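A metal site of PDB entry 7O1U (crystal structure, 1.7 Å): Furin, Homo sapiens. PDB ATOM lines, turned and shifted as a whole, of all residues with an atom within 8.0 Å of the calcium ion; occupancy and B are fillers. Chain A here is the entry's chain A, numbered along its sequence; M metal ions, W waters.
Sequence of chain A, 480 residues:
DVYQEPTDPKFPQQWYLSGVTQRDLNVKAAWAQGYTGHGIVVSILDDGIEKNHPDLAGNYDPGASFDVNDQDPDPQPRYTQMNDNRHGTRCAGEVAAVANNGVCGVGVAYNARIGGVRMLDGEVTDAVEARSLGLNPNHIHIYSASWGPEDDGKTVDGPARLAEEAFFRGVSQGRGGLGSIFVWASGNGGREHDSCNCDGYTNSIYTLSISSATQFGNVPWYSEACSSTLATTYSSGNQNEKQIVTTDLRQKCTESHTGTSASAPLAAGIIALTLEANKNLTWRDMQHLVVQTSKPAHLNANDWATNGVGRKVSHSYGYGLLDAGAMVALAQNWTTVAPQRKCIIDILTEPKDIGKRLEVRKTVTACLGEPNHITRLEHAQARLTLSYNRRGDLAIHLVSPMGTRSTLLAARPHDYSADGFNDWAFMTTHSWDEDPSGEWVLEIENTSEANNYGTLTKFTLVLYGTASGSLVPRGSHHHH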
ATOM      1  N   LYS A  51     -21.376  30.413  -9.830  1.00  0.00           N
ATOM      2  CA  LYS A  51     -21.118  31.316 -10.950  1.00  0.00           C
ATOM      3  C   LYS A  51     -22.221  31.280 -11.993  1.00  0.00           C
ATOM      4  O   LYS A  51     -22.351  32.238 -12.774  1.00  0.00           O
ATOM      5  CB  LYS A  51     -19.770  30.981 -11.591  1.00  0.00           C
ATOM      6  CG  LYS A  51     -19.693  29.627 -12.280  1.00  0.00           C
ATOM      7  CD  LYS A  51     -18.265  29.276 -12.698  1.00  0.00           C
ATOM      8  CE  LYS A  51     -18.186  27.908 -13.370  1.00  0.00           C
ATOM      9  NZ  LYS A  51     -18.469  26.781 -12.425  1.00  0.00           N
ATOM     10  N   PHE A  66     -10.967  31.704  -8.161  1.00  0.00           N
ATOM     11  CA  PHE A  66     -10.073  30.548  -8.078  1.00  0.00           C
ATOM     12  C   PHE A  66     -10.608  29.629  -6.987  1.00  0.00           C
ATOM     13  O   PHE A  66     -11.379  30.049  -6.120  1.00  0.00           O
ATOM     14  CB  PHE A  66      -8.623  30.958  -7.795  1.00  0.00           C
ATOM     15  CG  PHE A  66      -7.611  29.951  -8.278  1.00  0.00           C
ATOM     16  CD1 PHE A  66      -7.272  29.902  -9.615  1.00  0.00           C
ATOM     17  CD2 PHE A  66      -7.033  29.053  -7.402  1.00  0.00           C
ATOM     18  CE1 PHE A  66      -6.355  28.953 -10.077  1.00  0.00           C
ATOM     19  CE2 PHE A  66      -6.125  28.115  -7.859  1.00  0.00           C
ATOM     20  CZ  PHE A  66      -5.785  28.065  -9.197  1.00  0.00           C
ATOM     21  N   ASP A  67     -10.195  28.376  -7.045  1.00  0.00           N
ATOM     22  CA  ASP A  67     -10.503  27.378  -6.021  1.00  0.00           C
ATOM     23  C   ASP A  67      -9.194  26.975  -5.360  1.00  0.00           C
ATOM     24  O   ASP A  67      -8.465  26.120  -5.867  1.00  0.00           O
ATOM     25  CB  ASP A  67     -11.239  26.194  -6.627  1.00  0.00           C
ATOM     26  CG  ASP A  67     -11.633  25.144  -5.592  1.00  0.00           C
ATOM     27  OD1 ASP A  67     -11.138  25.188  -4.448  1.00  0.00           O
ATOM     28  OD2 ASP A  67     -12.441  24.272  -5.949  1.00  0.00           O
ATOM     29  N   VAL A  68      -8.898  27.609  -4.227  1.00  0.00           N
ATOM     30  CA  VAL A  68      -7.673  27.294  -3.498  1.00  0.00           C
ATOM     31  C   VAL A  68      -7.816  25.988  -2.741  1.00  0.00           C
ATOM     32  O   VAL A  68      -6.820  25.279  -2.551  1.00  0.00           O
ATOM     33  CB  VAL A  68      -7.330  28.467  -2.560  1.00  0.00           C
ATOM     34  CG1 VAL A  68      -6.092  28.163  -1.754  1.00  0.00           C
ATOM     35  CG2 VAL A  68      -7.124  29.731  -3.375  1.00  0.00           C
ATOM     36  N   ASN A  69      -9.025  25.630  -2.301  1.00  0.00           N
ATOM     37  CA  ASN A  69      -9.187  24.391  -1.540  1.00  0.00           C
ATOM     38  C   ASN A  69      -8.882  23.153  -2.380  1.00  0.00           C
ATOM     39  O   ASN A  69      -8.264  22.207  -1.887  1.00  0.00           O
ATOM     40  CB  ASN A  69     -10.604  24.284  -0.976  1.00  0.00           C
ATOM     41  CG  ASN A  69     -10.919  25.345   0.057  1.00  0.00           C
ATOM     42  OD1 ASN A  69     -11.937  26.019  -0.027  1.00  0.00           O
ATOM     43  ND2 ASN A  69     -10.047  25.476   1.065  1.00  0.00           N
ATOM     44  N   ASP A  70      -9.320  23.139  -3.643  1.00  0.00           N
ATOM     45  CA  ASP A  70      -9.084  21.999  -4.519  1.00  0.00           C
ATOM     46  C   ASP A  70      -8.037  22.276  -5.587  1.00  0.00           C
ATOM     47  O   ASP A  70      -7.739  21.391  -6.394  1.00  0.00           O
ATOM     48  CB  ASP A  70     -10.387  21.568  -5.213  1.00  0.00           C
ATOM     49  CG  ASP A  70     -11.295  20.735  -4.313  1.00  0.00           C
ATOM     50  OD1 ASP A  70     -10.841  20.298  -3.229  1.00  0.00           O
ATOM     51  OD2 ASP A  70     -12.469  20.520  -4.681  1.00  0.00           O
ATOM     52  N   GLN A  71      -7.478  23.491  -5.618  1.00  0.00           N
ATOM     53  CA  GLN A  71      -6.425  23.876  -6.559  1.00  0.00           C
ATOM     54  C   GLN A  71      -6.888  23.704  -8.007  1.00  0.00           C
ATOM     55  O   GLN A  71      -6.358  22.897  -8.769  1.00  0.00           O
ATOM     56  CB  GLN A  71      -5.139  23.079  -6.276  1.00  0.00           C
ATOM     57  CG  GLN A  71      -4.493  23.410  -4.934  1.00  0.00           C
ATOM     58  CD  GLN A  71      -3.312  22.505  -4.597  1.00  0.00           C
ATOM     59  N   ASP A  72      -7.876  24.499  -8.376  1.00  0.00           N
ATOM     60  CA  ASP A  72      -8.355  24.566  -9.749  1.00  0.00           C
ATOM     61  C   ASP A  72      -8.988  25.927  -9.954  1.00  0.00           C
ATOM     62  O   ASP A  72      -9.176  26.696  -8.997  1.00  0.00           O
ATOM     63  CB  ASP A  72      -9.338  23.427 -10.070  1.00  0.00           C
ATOM     64  CG  ASP A  72     -10.671  23.540  -9.317  1.00  0.00           C
ATOM     65  OD1 ASP A  72     -11.439  24.477  -9.584  1.00  0.00           O
ATOM     66  OD2 ASP A  72     -10.967  22.656  -8.491  1.00  0.00           O
ATOM     67  N   PRO A  73      -9.301  26.291 -11.208  1.00  0.00           N
ATOM     68  CA  PRO A  73      -9.795  27.650 -11.473  1.00  0.00           C
ATOM     69  C   PRO A  73     -11.245  27.876 -11.115  1.00  0.00           C
ATOM     70  O   PRO A  73     -11.674  29.034 -11.087  1.00  0.00           O
ATOM     71  CB  PRO A  73      -9.598  27.816 -12.999  1.00  0.00           C
ATOM     72  CG  PRO A  73      -8.754  26.678 -13.422  1.00  0.00           C
ATOM     73  CD  PRO A  73      -9.015  25.560 -12.455  1.00  0.00           C
ATOM     74  N   ASP A  74     -12.005  26.816 -10.831  1.00  0.00           N
ATOM     75  CA  ASP A  74     -13.470  26.870 -10.779  1.00  0.00           C
ATOM     76  C   ASP A  74     -13.960  26.937  -9.345  1.00  0.00           C
ATOM     77  O   ASP A  74     -13.869  25.943  -8.626  1.00  0.00           O
ATOM     78  CB  ASP A  74     -14.039  25.648 -11.489  1.00  0.00           C
ATOM     79  CG  ASP A  74     -15.556  25.595 -11.485  1.00  0.00           C
ATOM     80  OD1 ASP A  74     -16.203  26.501 -10.920  1.00  0.00           O
ATOM     81  OD2 ASP A  74     -16.106  24.640 -12.071  1.00  0.00           O
ATOM     82  N   PRO A  75     -14.522  28.089  -8.900  1.00  0.00           N
ATOM     83  CA  PRO A  75     -14.883  28.243  -7.486  1.00  0.00           C
ATOM     84  C   PRO A  75     -16.267  27.731  -7.118  1.00  0.00           C
ATOM     85  O   PRO A  75     -16.805  28.120  -6.076  1.00  0.00           O
ATOM     86  CB  PRO A  75     -14.825  29.770  -7.287  1.00  0.00           C
ATOM     87  CG  PRO A  75     -15.399  30.252  -8.602  1.00  0.00           C
ATOM     88  CD  PRO A  75     -14.756  29.351  -9.643  1.00  0.00           C
ATOM     89  N   GLN A  76     -16.863  26.905  -7.964  1.00  0.00           N
ATOM     90  CA  GLN A  76     -18.234  26.453  -7.715  1.00  0.00           C
ATOM     91  C   GLN A  76     -18.329  25.848  -6.320  1.00  0.00           C
ATOM     92  O   GLN A  76     -17.460  25.060  -5.917  1.00  0.00           O
ATOM     93  CB  GLN A  76     -18.666  25.416  -8.760  1.00  0.00           C
ATOM     94  CG  GLN A  76     -20.176  25.162  -8.800  1.00  0.00           C
ATOM     95  CD  GLN A  76     -20.951  26.250  -9.515  1.00  0.00           C
ATOM     96  OE1 GLN A  76     -20.377  27.050 -10.256  1.00  0.00           O
ATOM     97  NE2 GLN A  76     -22.262  26.277  -9.314  1.00  0.00           N
ATOM     98  N   PRO A  77     -19.372  26.168  -5.551  1.00  0.00           N
ATOM     99  CA  PRO A  77     -19.476  25.607  -4.200  1.00  0.00           C
ATOM    100  C   PRO A  77     -19.715  24.109  -4.215  1.00  0.00           C
ATOM    101  O   PRO A  77     -20.265  23.537  -5.159  1.00  0.00           O
ATOM    102  CB  PRO A  77     -20.670  26.337  -3.586  1.00  0.00           C
ATOM    103  CG  PRO A  77     -20.907  27.535  -4.468  1.00  0.00           C
ATOM    104  CD  PRO A  77     -20.471  27.108  -5.838  1.00  0.00           C
ATOM    105  N   ARG A  78     -19.310  23.464  -3.122  1.00  0.00           N
ATOM    106  CA  ARG A  78     -19.621  22.070  -2.850  1.00  0.00           C
ATOM    107  C   ARG A  78     -21.044  21.963  -2.302  1.00  0.00           C
ATOM    108  O   ARG A  78     -21.341  22.509  -1.235  1.00  0.00           O
ATOM    109  CB  ARG A  78     -18.598  21.495  -1.875  1.00  0.00           C
ATOM    110  CG  ARG A  78     -18.802  20.017  -1.525  1.00  0.00           C
ATOM    111  CD  ARG A  78     -17.676  19.498  -0.613  1.00  0.00           C
ATOM    112  NE  ARG A  78     -17.578  20.292   0.605  1.00  0.00           N
ATOM    113  CZ  ARG A  78     -18.203  20.006   1.751  1.00  0.00           C
ATOM    114  NH1 ARG A  78     -18.067  20.817   2.795  1.00  0.00           N
ATOM    115  NH2 ARG A  78     -18.948  18.918   1.861  1.00  0.00           N
ATOM    116  N   ARG A 118     -12.829  30.136  -3.642  1.00  0.00           N
ATOM    117  CA  ARG A 118     -13.232  29.037  -2.779  1.00  0.00           C
ATOM    118  C   ARG A 118     -12.009  28.688  -1.933  1.00  0.00           C
ATOM    119  O   ARG A 118     -11.055  28.085  -2.428  1.00  0.00           O
ATOM    120  CB  ARG A 118     -13.727  27.860  -3.614  1.00  0.00           C
ATOM    121  CG  ARG A 118     -14.234  26.680  -2.802  1.00  0.00           C
ATOM    122  CD  ARG A 118     -14.885  25.585  -3.685  1.00  0.00           C
ATOM    123  NE  ARG A 118     -15.234  24.450  -2.839  1.00  0.00           N
ATOM    124  CZ  ARG A 118     -14.587  23.296  -2.796  1.00  0.00           C
ATOM    125  NH1 ARG A 118     -14.979  22.365  -1.942  1.00  0.00           N
ATOM    126  NH2 ARG A 118     -13.568  23.048  -3.614  1.00  0.00           N
HETATM  127 CA    CA M   1     -13.279  23.650  -8.043  1.00  0.00          CA
HETATM  128  O   HOH W   1     -13.550  21.461  -7.046  1.00  0.00           O
HETATM  129  O   HOH W   2     -14.228  22.472  -9.974  1.00  0.00           O
HETATM  130  O   HOH W   3     -15.541  23.664  -7.399  1.00  0.00           O
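The side-chain carboxylate of Asp 67 lies within salt-bridge range of the guanidinium group of Arg 118 (3.3 Å). The side-chain carboxylate (OD1) of Asp 67 is in hydrogen-bond range of the backbone NH (N) of Asp 70. OD1 of Asp 67 sits at hydrogen-bond distance from N of Asn 69, at 3.0 Å. N of Gln 76 is in hydrogen-bond range of OD1 of Asp 74, at 3.1 Å. The side-chain carboxylate of Asp 74 lies within salt-bridge range of the side-chain amino group of Lys 51.
The calcium ion is bound by the side-chain carboxylate (OD2) of Asp 67, water W3, water W1, the backbone carbonyl oxygen (O) of Asp 74, water W2, the side-chain carboxylate (OD1) of Asp 72 and the side-chain carboxylate (OD2) of Asp 72.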
